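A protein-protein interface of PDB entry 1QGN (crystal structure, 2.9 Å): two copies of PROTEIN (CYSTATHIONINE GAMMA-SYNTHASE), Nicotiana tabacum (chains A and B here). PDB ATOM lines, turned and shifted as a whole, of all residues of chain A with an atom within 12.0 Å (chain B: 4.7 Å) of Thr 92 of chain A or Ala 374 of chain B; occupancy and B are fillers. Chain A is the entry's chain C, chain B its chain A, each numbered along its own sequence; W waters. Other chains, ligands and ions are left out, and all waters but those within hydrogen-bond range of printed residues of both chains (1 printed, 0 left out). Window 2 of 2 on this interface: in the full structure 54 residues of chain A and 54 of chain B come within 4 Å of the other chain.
OD1 of Asp 378 of chain B lies within hydrogen-bond range of OG1 of Thr 92 of chain A (2.7 Å).
The backbone NH of Phe 89 of chain A sits at hydrogen-bond distance from the backbone carbonyl oxygen of Ile 385 of chain B (2.9 Å).
Printed residues of chain B within 4 Å of Phe 89 of chain A: Ile 385 (2.9 Å).
Of the printed residues of chain B, Lys 91 of chain A touches Asp 378 (3.4 Å) and Ile 385 (3.9 Å).
Thr 92 of chain A touches just these residues of chain B: Ala 374, Val 377, Asp 378, Ile 385 and Ile 401.
No residue of chain A comes within 4 Å of Thr 372 of chain B.
Of chain A, only Thr 92 (3.9 Å) comes within 4 Å of Ala 374 of chain B.
No residue of chain A comes within 4 Å of Lys 375 of chain B.
Of chain A, only Lys 91 and Thr 92 come within 4 Å of Asp 378 of chain B.
Ile 385 of chain B touches four residues of chain A.
No residue of chain A comes within 4 Å of Gln 398 of chain B.
Ile 401 of chain B touches just these residues of chain A: Thr 92 (3.4 Å), Leu 95 (3.4 Å) and Lys 99 (3.8 Å).
Among the printed residues, merely in contact across the chains: Phe 88 of chain A with Ile 385 of chain B (3.3 Å), Lys 91 of chain A with Asp 378 of chain B (3.4 Å), Lys 91 of chain A with Ile 385 of chain B (3.9 Å), Thr 92 of chain A with Ala 374 of chain B (3.9 Å), Thr 92 of chain A with Val 377 of chain B (3.5 Å), Thr 92 of chain A with Ile 385 of chain B (3.9 Å), Thr 92 of chain A with Ile 401 of chain B (3.4 Å), Leu 95 of chain A with Ile 401 of chain B (3.4 Å) and Lys 99 of chain A with Ile 401 of chain B (3.8 Å).
Of the 20 printed residues of chain A, 6 touch a printed residue of chain B.
Hydrophobic or aromatic side chains of chain A within 4 Å of the printed part of chain B: Phe 88, Phe 89 and Leu 95.
Printed residues of chain B that touch a printed residue of chain A: Ala 374, Val 377, Asp 378, Ile 385 and Ile 401.
Hydrophobic or aromatic side chains of chain B within 4 Å of the printed part of chain A: Ala 374, Val 377, Ile 385 and Ile 401.
Among the printed residues, 11 pairs touch across the chains.
Among the printed residues, no Asp or Glu carboxylate lies within 4 Å of a Lys or Arg side-chain nitrogen of the other chain.
No position is printed for both chains.
NZ of Lys 99 of chain A is in salt-bridge range of OE2 of Glu 107 of chain A (3.0 Å).
Water W1 lies within hydrogen-bond range of the side-chain hydroxyl (OG1) of Thr 92 of chain A (2.5 Å) and the side-chain amide oxygen (OE1) of Gln 398 of chain B (3.3 Å).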
ATOM      1  N   TYR A  87     -17.384 -29.960   7.057  1.00  0.00           N
ATOM      2  CA  TYR A  87     -16.784 -28.722   7.529  1.00  0.00           C
ATOM      3  C   TYR A  87     -17.659 -28.205   8.660  1.00  0.00           C
ATOM      4  O   TYR A  87     -18.883 -28.273   8.587  1.00  0.00           O
ATOM      5  CB  TYR A  87     -16.694 -27.716   6.368  1.00  0.00           C
ATOM      6  CG  TYR A  87     -15.961 -28.289   5.161  1.00  0.00           C
ATOM      7  CD1 TYR A  87     -16.638 -29.046   4.197  1.00  0.00           C
ATOM      8  CD2 TYR A  87     -14.580 -28.146   5.024  1.00  0.00           C
ATOM      9  CE1 TYR A  87     -15.955 -29.646   3.138  1.00  0.00           C
ATOM     10  CE2 TYR A  87     -13.894 -28.746   3.968  1.00  0.00           C
ATOM     11  CZ  TYR A  87     -14.585 -29.492   3.037  1.00  0.00           C
ATOM     12  OH  TYR A  87     -13.900 -30.111   2.017  1.00  0.00           O
ATOM     13  N   PHE A  88     -17.037 -27.698   9.715  1.00  0.00           N
ATOM     14  CA  PHE A  88     -17.801 -27.225  10.850  1.00  0.00           C
ATOM     15  C   PHE A  88     -18.004 -25.728  10.902  1.00  0.00           C
ATOM     16  O   PHE A  88     -17.343 -24.973  10.193  1.00  0.00           O
ATOM     17  CB  PHE A  88     -17.126 -27.675  12.138  1.00  0.00           C
ATOM     18  CG  PHE A  88     -15.833 -26.974  12.417  1.00  0.00           C
ATOM     19  CD1 PHE A  88     -15.812 -25.789  13.134  1.00  0.00           C
ATOM     20  CD2 PHE A  88     -14.630 -27.516  11.994  1.00  0.00           C
ATOM     21  CE1 PHE A  88     -14.607 -25.149  13.436  1.00  0.00           C
ATOM     22  CE2 PHE A  88     -13.421 -26.883  12.291  1.00  0.00           C
ATOM     23  CZ  PHE A  88     -13.414 -25.696  13.016  1.00  0.00           C
ATOM     24  N   PHE A  89     -18.922 -25.314  11.773  1.00  0.00           N
ATOM     25  CA  PHE A  89     -19.251 -23.909  11.980  1.00  0.00           C
ATOM     26  C   PHE A  89     -19.008 -23.578  13.451  1.00  0.00           C
ATOM     27  O   PHE A  89     -19.212 -24.421  14.318  1.00  0.00           O
ATOM     28  CB  PHE A  89     -20.711 -23.655  11.596  1.00  0.00           C
ATOM     29  CG  PHE A  89     -21.022 -23.993  10.161  1.00  0.00           C
ATOM     30  CD1 PHE A  89     -21.160 -25.318   9.760  1.00  0.00           C
ATOM     31  CD2 PHE A  89     -21.138 -22.995   9.201  1.00  0.00           C
ATOM     32  CE1 PHE A  89     -21.405 -25.647   8.425  1.00  0.00           C
ATOM     33  CE2 PHE A  89     -21.384 -23.317   7.858  1.00  0.00           C
ATOM     34  CZ  PHE A  89     -21.516 -24.648   7.474  1.00  0.00           C
ATOM     35  N   ASN A  90     -18.555 -22.361  13.729  1.00  0.00           N
ATOM     36  CA  ASN A  90     -18.269 -21.946  15.097  1.00  0.00           C
ATOM     37  C   ASN A  90     -19.495 -21.777  15.978  1.00  0.00           C
ATOM     38  O   ASN A  90     -19.439 -22.038  17.178  1.00  0.00           O
ATOM     39  CB  ASN A  90     -17.484 -20.646  15.086  1.00  0.00           C
ATOM     40  CG  ASN A  90     -16.167 -20.785  14.384  1.00  0.00           C
ATOM     41  OD1 ASN A  90     -15.229 -21.382  14.916  1.00  0.00           O
ATOM     42  ND2 ASN A  90     -16.084 -20.243  13.176  1.00  0.00           N
ATOM     43  N   LYS A  91     -20.592 -21.312  15.392  1.00  0.00           N
ATOM     44  CA  LYS A  91     -21.826 -21.125  16.138  1.00  0.00           C
ATOM     45  C   LYS A  91     -22.987 -21.090  15.170  1.00  0.00           C
ATOM     46  O   LYS A  91     -22.827 -20.696  14.019  1.00  0.00           O
ATOM     47  CB  LYS A  91     -21.786 -19.829  16.941  1.00  0.00           C
ATOM     48  CG  LYS A  91     -20.809 -18.803  16.423  1.00  0.00           C
ATOM     49  CD  LYS A  91     -21.127 -17.428  16.989  1.00  0.00           C
ATOM     50  CE  LYS A  91     -19.872 -16.575  17.139  1.00  0.00           C
ATOM     51  NZ  LYS A  91     -20.034 -15.510  18.174  1.00  0.00           N
ATOM     52  N   THR A  92     -24.154 -21.512  15.637  1.00  0.00           N
ATOM     53  CA  THR A  92     -25.338 -21.539  14.800  1.00  0.00           C
ATOM     54  C   THR A  92     -25.484 -20.243  14.031  1.00  0.00           C
ATOM     55  O   THR A  92     -25.931 -20.240  12.887  1.00  0.00           O
ATOM     56  CB  THR A  92     -26.582 -21.773  15.641  1.00  0.00           C
ATOM     57  OG1 THR A  92     -26.374 -22.925  16.461  1.00  0.00           O
ATOM     58  CG2 THR A  92     -27.796 -22.009  14.753  1.00  0.00           C
ATOM     59  N   SER A  93     -25.095 -19.140  14.661  1.00  0.00           N
ATOM     60  CA  SER A  93     -25.178 -17.825  14.026  1.00  0.00           C
ATOM     61  C   SER A  93     -24.488 -17.838  12.662  1.00  0.00           C
ATOM     62  O   SER A  93     -25.088 -17.478  11.650  1.00  0.00           O
ATOM     63  CB  SER A  93     -24.533 -16.761  14.924  1.00  0.00           C
ATOM     64  OG  SER A  93     -23.495 -16.070  14.247  1.00  0.00           O
ATOM     65  N   GLU A  94     -23.226 -18.261  12.644  1.00  0.00           N
ATOM     66  CA  GLU A  94     -22.449 -18.322  11.416  1.00  0.00           C
ATOM     67  C   GLU A  94     -22.996 -19.332  10.421  1.00  0.00           C
ATOM     68  O   GLU A  94     -22.822 -19.174   9.215  1.00  0.00           O
ATOM     69  CB  GLU A  94     -20.999 -18.640  11.744  1.00  0.00           C
ATOM     70  CG  GLU A  94     -20.374 -17.594  12.644  1.00  0.00           C
ATOM     71  CD  GLU A  94     -18.923 -17.888  12.964  1.00  0.00           C
ATOM     72  OE1 GLU A  94     -18.410 -18.931  12.500  1.00  0.00           O
ATOM     73  OE2 GLU A  94     -18.298 -17.073  13.684  1.00  0.00           O
ATOM     74  N   LEU A  95     -23.662 -20.367  10.916  1.00  0.00           N
ATOM     75  CA  LEU A  95     -24.232 -21.371  10.028  1.00  0.00           C
ATOM     76  C   LEU A  95     -25.366 -20.736   9.228  1.00  0.00           C
ATOM     77  O   LEU A  95     -25.539 -21.013   8.040  1.00  0.00           O
ATOM     78  CB  LEU A  95     -24.763 -22.563  10.831  1.00  0.00           C
ATOM     79  CG  LEU A  95     -25.670 -23.532  10.065  1.00  0.00           C
ATOM     80  CD1 LEU A  95     -24.926 -24.181   8.898  1.00  0.00           C
ATOM     81  CD2 LEU A  95     -26.159 -24.580  11.025  1.00  0.00           C
ATOM     82  N   ILE A  96     -26.137 -19.878   9.890  1.00  0.00           N
ATOM     83  CA  ILE A  96     -27.248 -19.196   9.241  1.00  0.00           C
ATOM     84  C   ILE A  96     -26.686 -18.214   8.221  1.00  0.00           C
ATOM     85  O   ILE A  96     -27.152 -18.168   7.087  1.00  0.00           O
ATOM     86  CB  ILE A  96     -28.121 -18.438  10.268  1.00  0.00           C
ATOM     87  CG1 ILE A  96     -28.898 -19.439  11.127  1.00  0.00           C
ATOM     88  CG2 ILE A  96     -29.100 -17.524   9.555  1.00  0.00           C
ATOM     89  CD1 ILE A  96     -29.528 -18.831  12.366  1.00  0.00           C
ATOM     90  N   ASP A  97     -25.688 -17.433   8.627  1.00  0.00           N
ATOM     91  CA  ASP A  97     -25.054 -16.482   7.723  1.00  0.00           C
ATOM     92  C   ASP A  97     -24.789 -17.201   6.415  1.00  0.00           C
ATOM     93  O   ASP A  97     -25.302 -16.823   5.364  1.00  0.00           O
ATOM     94  CB  ASP A  97     -23.725 -16.011   8.294  1.00  0.00           C
ATOM     95  CG  ASP A  97     -23.886 -14.877   9.265  1.00  0.00           C
ATOM     96  OD1 ASP A  97     -25.000 -14.313   9.342  1.00  0.00           O
ATOM     97  OD2 ASP A  97     -22.895 -14.550   9.950  1.00  0.00           O
ATOM     98  N   PHE A  98     -23.986 -18.254   6.502  1.00  0.00           N
ATOM     99  CA  PHE A  98     -23.637 -19.058   5.346  1.00  0.00           C
ATOM    100  C   PHE A  98     -24.882 -19.503   4.584  1.00  0.00           C
ATOM    101  O   PHE A  98     -24.914 -19.476   3.353  1.00  0.00           O
ATOM    102  CB  PHE A  98     -22.828 -20.281   5.794  1.00  0.00           C
ATOM    103  CG  PHE A  98     -22.933 -21.454   4.860  1.00  0.00           C
ATOM    104  CD1 PHE A  98     -22.340 -21.417   3.606  1.00  0.00           C
ATOM    105  CD2 PHE A  98     -23.644 -22.588   5.230  1.00  0.00           C
ATOM    106  CE1 PHE A  98     -22.457 -22.493   2.730  1.00  0.00           C
ATOM    107  CE2 PHE A  98     -23.767 -23.667   4.361  1.00  0.00           C
ATOM    108  CZ  PHE A  98     -23.172 -23.619   3.108  1.00  0.00           C
ATOM    109  N   LYS A  99     -25.912 -19.909   5.314  1.00  0.00           N
ATOM    110  CA  LYS A  99     -27.139 -20.369   4.682  1.00  0.00           C
ATOM    111  C   LYS A  99     -27.854 -19.245   3.936  1.00  0.00           C
ATOM    112  O   LYS A  99     -28.602 -19.488   2.986  1.00  0.00           O
ATOM    113  CB  LYS A  99     -28.060 -20.976   5.738  1.00  0.00           C
ATOM    114  CG  LYS A  99     -27.683 -22.397   6.109  1.00  0.00           C
ATOM    115  CD  LYS A  99     -27.893 -23.331   4.931  1.00  0.00           C
ATOM    116  CE  LYS A  99     -27.251 -24.681   5.168  1.00  0.00           C
ATOM    117  NZ  LYS A  99     -28.004 -25.745   4.445  1.00  0.00           N
ATOM    118  N   GLU A 100     -27.612 -18.013   4.370  1.00  0.00           N
ATOM    119  CA  GLU A 100     -28.229 -16.841   3.753  1.00  0.00           C
ATOM    120  C   GLU A 100     -27.223 -16.140   2.845  1.00  0.00           C
ATOM    121  O   GLU A 100     -27.340 -14.947   2.557  1.00  0.00           O
ATOM    122  CB  GLU A 100     -28.730 -15.883   4.838  1.00  0.00           C
ATOM    123  CG  GLU A 100     -29.352 -16.595   6.028  1.00  0.00           C
ATOM    124  CD  GLU A 100     -30.604 -15.913   6.541  1.00  0.00           C
ATOM    125  OE1 GLU A 100     -30.501 -14.755   7.000  1.00  0.00           O
ATOM    126  OE2 GLU A 100     -31.689 -16.537   6.489  1.00  0.00           O
ATOM    127  N   LYS A 101     -26.231 -16.909   2.409  1.00  0.00           N
ATOM    128  CA  LYS A 101     -25.190 -16.423   1.520  1.00  0.00           C
ATOM    129  C   LYS A 101     -24.420 -15.224   2.056  1.00  0.00           C
ATOM    130  O   LYS A 101     -23.957 -14.387   1.287  1.00  0.00           O
ATOM    131  CB  LYS A 101     -25.795 -16.087   0.159  1.00  0.00           C
ATOM    132  CG  LYS A 101     -26.122 -17.307  -0.686  1.00  0.00           C
ATOM    133  CD  LYS A 101     -27.401 -17.980  -0.214  1.00  0.00           C
ATOM    134  CE  LYS A 101     -27.923 -18.961  -1.254  1.00  0.00           C
ATOM    135  NZ  LYS A 101     -28.297 -18.279  -2.529  1.00  0.00           N
ATOM    136  N   ARG A 102     -24.275 -15.139   3.371  1.00  0.00           N
ATOM    137  CA  ARG A 102     -23.539 -14.036   3.976  1.00  0.00           C
ATOM    138  C   ARG A 102     -22.161 -14.521   4.412  1.00  0.00           C
ATOM    139  O   ARG A 102     -21.331 -13.743   4.888  1.00  0.00           O
ATOM    140  CB  ARG A 102     -24.298 -13.486   5.179  1.00  0.00           C
ATOM    141  CG  ARG A 102     -25.290 -12.400   4.833  1.00  0.00           C
ATOM    142  CD  ARG A 102     -25.721 -11.644   6.070  1.00  0.00           C
ATOM    143  NE  ARG A 102     -26.226 -12.536   7.112  1.00  0.00           N
ATOM    144  CZ  ARG A 102     -27.368 -13.213   7.031  1.00  0.00           C
ATOM    145  NH1 ARG A 102     -28.134 -13.102   5.953  1.00  0.00           N
ATOM    146  NH2 ARG A 102     -27.744 -13.999   8.030  1.00  0.00           N
ATOM    147  N   ARG A 103     -21.936 -15.822   4.255  1.00  0.00           N
ATOM    148  CA  ARG A 103     -20.669 -16.453   4.601  1.00  0.00           C
ATOM    149  C   ARG A 103     -20.408 -17.577   3.593  1.00  0.00           C
ATOM    150  O   ARG A 103     -21.329 -18.038   2.910  1.00  0.00           O
ATOM    151  CB  ARG A 103     -20.716 -17.022   6.026  1.00  0.00           C
ATOM    152  CG  ARG A 103     -19.531 -17.928   6.349  1.00  0.00           C
ATOM    153  CD  ARG A 103     -19.582 -18.492   7.753  1.00  0.00           C
ATOM    154  NE  ARG A 103     -18.651 -17.796   8.633  1.00  0.00           N
ATOM    155  CZ  ARG A 103     -18.860 -16.572   9.106  1.00  0.00           C
ATOM    156  NH1 ARG A 103     -19.969 -15.910   8.781  1.00  0.00           N
ATOM    157  NH2 ARG A 103     -17.963 -16.004   9.905  1.00  0.00           N
ATOM    158  N   ALA A 104     -19.156 -18.014   3.498  1.00  0.00           N
ATOM    159  CA  ALA A 104     -18.801 -19.076   2.567  1.00  0.00           C
ATOM    160  C   ALA A 104     -18.358 -20.351   3.274  1.00  0.00           C
ATOM    161  O   ALA A 104     -17.690 -20.306   4.311  1.00  0.00           O
ATOM    162  CB  ALA A 104     -17.701 -18.598   1.634  1.00  0.00           C
ATOM    163  N   SER A 105     -18.734 -21.489   2.699  1.00  0.00           N
ATOM    164  CA  SER A 105     -18.373 -22.785   3.250  1.00  0.00           C
ATOM    165  C   SER A 105     -18.763 -23.883   2.272  1.00  0.00           C
ATOM    166  O   SER A 105     -19.689 -23.717   1.476  1.00  0.00           O
ATOM    167  CB  SER A 105     -19.083 -23.014   4.587  1.00  0.00           C
ATOM    168  OG  SER A 105     -19.083 -24.387   4.948  1.00  0.00           O
ATOM    169  N   GLU A 107     -19.520 -26.761   3.468  1.00  0.00           N
ATOM    170  CA  GLU A 107     -20.483 -27.457   4.316  1.00  0.00           C
ATOM    171  C   GLU A 107     -20.221 -28.952   4.353  1.00  0.00           C
ATOM    172  O   GLU A 107     -19.770 -29.483   5.361  1.00  0.00           O
ATOM    173  CB  GLU A 107     -21.908 -27.207   3.827  1.00  0.00           C
ATOM    174  CG  GLU A 107     -22.962 -27.339   4.905  1.00  0.00           C
ATOM    175  CD  GLU A 107     -24.323 -27.703   4.346  1.00  0.00           C
ATOM    176  OE1 GLU A 107     -24.539 -28.878   3.987  1.00  0.00           O
ATOM    177  OE2 GLU A 107     -25.189 -26.815   4.262  1.00  0.00           O
ATOM    178  N   ASP B 369     -37.200 -22.853  21.377  1.00  0.00           N
ATOM    179  CA  ASP B 369     -37.442 -22.495  19.984  1.00  0.00           C
ATOM    180  C   ASP B 369     -36.135 -22.474  19.186  1.00  0.00           C
ATOM    181  O   ASP B 369     -35.064 -22.775  19.721  1.00  0.00           O
ATOM    182  CB  ASP B 369     -38.133 -21.125  19.901  1.00  0.00           C
ATOM    183  CG  ASP B 369     -37.340 -20.024  20.590  1.00  0.00           C
ATOM    184  OD1 ASP B 369     -36.459 -20.336  21.419  1.00  0.00           O
ATOM    185  OD2 ASP B 369     -37.600 -18.837  20.302  1.00  0.00           O
ATOM    186  N   LEU B 370     -36.230 -22.128  17.906  1.00  0.00           N
ATOM    187  CA  LEU B 370     -35.068 -22.068  17.041  1.00  0.00           C
ATOM    188  C   LEU B 370     -33.908 -21.444  17.797  1.00  0.00           C
ATOM    189  O   LEU B 370     -32.834 -22.029  17.910  1.00  0.00           O
ATOM    190  CB  LEU B 370     -35.394 -21.232  15.800  1.00  0.00           C
ATOM    191  CG  LEU B 370     -34.570 -21.371  14.508  1.00  0.00           C
ATOM    192  CD1 LEU B 370     -33.346 -20.486  14.610  1.00  0.00           C
ATOM    193  CD2 LEU B 370     -34.171 -22.816  14.260  1.00  0.00           C
ATOM    194  N   LEU B 371     -34.148 -20.261  18.341  1.00  0.00           N
ATOM    195  CA  LEU B 371     -33.128 -19.526  19.074  1.00  0.00           C
ATOM    196  C   LEU B 371     -32.613 -20.191  20.340  1.00  0.00           C
ATOM    197  O   LEU B 371     -31.409 -20.226  20.573  1.00  0.00           O
ATOM    198  CB  LEU B 371     -33.648 -18.132  19.421  1.00  0.00           C
ATOM    199  CG  LEU B 371     -33.131 -16.987  18.550  1.00  0.00           C
ATOM    200  CD1 LEU B 371     -31.711 -16.641  18.980  1.00  0.00           C
ATOM    201  CD2 LEU B 371     -33.171 -17.388  17.072  1.00  0.00           C
ATOM    202  N   THR B 372     -33.523 -20.696  21.167  1.00  0.00           N
ATOM    203  CA  THR B 372     -33.142 -21.352  22.419  1.00  0.00           C
ATOM    204  C   THR B 372     -32.387 -22.642  22.131  1.00  0.00           C
ATOM    205  O   THR B 372     -31.320 -22.885  22.698  1.00  0.00           O
ATOM    206  CB  THR B 372     -34.380 -21.675  23.285  1.00  0.00           C
ATOM    207  OG1 THR B 372     -34.890 -20.464  23.858  1.00  0.00           O
ATOM    208  CG2 THR B 372     -34.016 -22.645  24.398  1.00  0.00           C
ATOM    209  N   THR B 373     -32.957 -23.472  21.262  1.00  0.00           N
ATOM    210  CA  THR B 373     -32.327 -24.724  20.879  1.00  0.00           C
ATOM    211  C   THR B 373     -30.911 -24.403  20.415  1.00  0.00           C
ATOM    212  O   THR B 373     -29.947 -25.076  20.789  1.00  0.00           O
ATOM    213  CB  THR B 373     -33.080 -25.392  19.717  1.00  0.00           C
ATOM    214  OG1 THR B 373     -34.459 -25.553  20.065  1.00  0.00           O
ATOM    215  CG2 THR B 373     -32.481 -26.745  19.411  1.00  0.00           C
ATOM    216  N   ALA B 374     -30.802 -23.358  19.599  1.00  0.00           N
ATOM    217  CA  ALA B 374     -29.520 -22.926  19.075  1.00  0.00           C
ATOM    218  C   ALA B 374     -28.572 -22.610  20.219  1.00  0.00           C
ATOM    219  O   ALA B 374     -27.428 -23.050  20.219  1.00  0.00           O
ATOM    220  CB  ALA B 374     -29.704 -21.707  18.200  1.00  0.00           C
ATOM    221  N   LYS B 375     -29.048 -21.854  21.199  1.00  0.00           N
ATOM    222  CA  LYS B 375     -28.218 -21.489  22.342  1.00  0.00           C
ATOM    223  C   LYS B 375     -27.625 -22.717  23.005  1.00  0.00           C
ATOM    224  O   LYS B 375     -26.521 -22.665  23.556  1.00  0.00           O
ATOM    225  CB  LYS B 375     -29.033 -20.708  23.371  1.00  0.00           C
ATOM    226  CG  LYS B 375     -28.181 -20.072  24.463  1.00  0.00           C
ATOM    227  CD  LYS B 375     -28.974 -19.875  25.748  1.00  0.00           C
ATOM    228  CE  LYS B 375     -29.183 -18.393  26.044  1.00  0.00           C
ATOM    229  NZ  LYS B 375     -30.039 -17.712  25.021  1.00  0.00           N
ATOM    230  N   PHE B 376     -28.371 -23.818  22.953  1.00  0.00           N
ATOM    231  CA  PHE B 376     -27.932 -25.079  23.535  1.00  0.00           C
ATOM    232  C   PHE B 376     -26.757 -25.654  22.753  1.00  0.00           C
ATOM    233  O   PHE B 376     -25.686 -25.882  23.319  1.00  0.00           O
ATOM    234  CB  PHE B 376     -29.086 -26.090  23.553  1.00  0.00           C
ATOM    235  CG  PHE B 376     -28.642 -27.530  23.675  1.00  0.00           C
ATOM    236  CD1 PHE B 376     -27.833 -27.946  24.737  1.00  0.00           C
ATOM    237  CD2 PHE B 376     -29.040 -28.476  22.725  1.00  0.00           C
ATOM    238  CE1 PHE B 376     -27.429 -29.278  24.848  1.00  0.00           C
ATOM    239  CE2 PHE B 376     -28.640 -29.809  22.830  1.00  0.00           C
ATOM    240  CZ  PHE B 376     -27.836 -30.209  23.893  1.00  0.00           C
ATOM    241  N   VAL B 377     -26.947 -25.881  21.454  1.00  0.00           N
ATOM    242  CA  VAL B 377     -25.875 -26.444  20.635  1.00  0.00           C
ATOM    243  C   VAL B 377     -24.661 -25.527  20.608  1.00  0.00           C
ATOM    244  O   VAL B 377     -23.534 -25.982  20.457  1.00  0.00           O
ATOM    245  CB  VAL B 377     -26.334 -26.741  19.180  1.00  0.00           C
ATOM    246  CG1 VAL B 377     -27.818 -26.554  19.050  1.00  0.00           C
ATOM    247  CG2 VAL B 377     -25.607 -25.857  18.213  1.00  0.00           C
ATOM    248  N   ASP B 378     -24.882 -24.234  20.757  1.00  0.00           N
ATOM    249  CA  ASP B 378     -23.758 -23.314  20.763  1.00  0.00           C
ATOM    250  C   ASP B 378     -22.995 -23.480  22.078  1.00  0.00           C
ATOM    251  O   ASP B 378     -21.807 -23.181  22.161  1.00  0.00           O
ATOM    252  CB  ASP B 378     -24.245 -21.866  20.632  1.00  0.00           C
ATOM    253  CG  ASP B 378     -24.409 -21.427  19.188  1.00  0.00           C
ATOM    254  OD1 ASP B 378     -24.465 -22.299  18.298  1.00  0.00           O
ATOM    255  OD2 ASP B 378     -24.483 -20.202  18.940  1.00  0.00           O
ATOM    256  N   ILE B 385     -20.254 -28.396  15.161  1.00  0.00           N
ATOM    257  CA  ILE B 385     -21.558 -28.111  14.583  1.00  0.00           C
ATOM    258  C   ILE B 385     -21.310 -28.355  13.101  1.00  0.00           C
ATOM    259  O   ILE B 385     -20.667 -27.544  12.442  1.00  0.00           O
ATOM    260  CB  ILE B 385     -21.971 -26.658  14.787  1.00  0.00           C
ATOM    261  CG1 ILE B 385     -21.870 -26.288  16.270  1.00  0.00           C
ATOM    262  CG2 ILE B 385     -23.387 -26.466  14.274  1.00  0.00           C
ATOM    263  CD1 ILE B 385     -22.526 -24.967  16.630  1.00  0.00           C
ATOM    264  N   GLN B 398     -28.752 -28.871  13.737  1.00  0.00           N
ATOM    265  CA  GLN B 398     -30.185 -28.637  13.818  1.00  0.00           C
ATOM    266  C   GLN B 398     -30.749 -28.853  12.419  1.00  0.00           C
ATOM    267  O   GLN B 398     -30.774 -27.930  11.610  1.00  0.00           O
ATOM    268  CB  GLN B 398     -30.440 -27.201  14.257  1.00  0.00           C
ATOM    269  CG  GLN B 398     -31.225 -27.050  15.540  1.00  0.00           C
ATOM    270  CD  GLN B 398     -31.201 -25.627  16.068  1.00  0.00           C
ATOM    271  OE1 GLN B 398     -30.133 -25.086  16.375  1.00  0.00           O
ATOM    272  NE2 GLN B 398     -32.378 -25.010  16.171  1.00  0.00           N
ATOM    273  N   ILE B 401     -32.122 -25.932  10.436  1.00  0.00           N
ATOM    274  CA  ILE B 401     -31.212 -24.933   9.898  1.00  0.00           C
ATOM    275  C   ILE B 401     -30.229 -25.539   8.906  1.00  0.00           C
ATOM    276  O   ILE B 401     -29.947 -24.956   7.863  1.00  0.00           O
ATOM    277  CB  ILE B 401     -30.393 -24.268  11.012  1.00  0.00           C
ATOM    278  CG1 ILE B 401     -31.313 -23.449  11.913  1.00  0.00           C
ATOM    279  CG2 ILE B 401     -29.325 -23.377  10.407  1.00  0.00           C
ATOM    280  CD1 ILE B 401     -30.586 -22.711  13.026  1.00  0.00           C
HETATM  281  O   HOH W   1     -27.028 -25.078  15.303  1.00  0.00           O
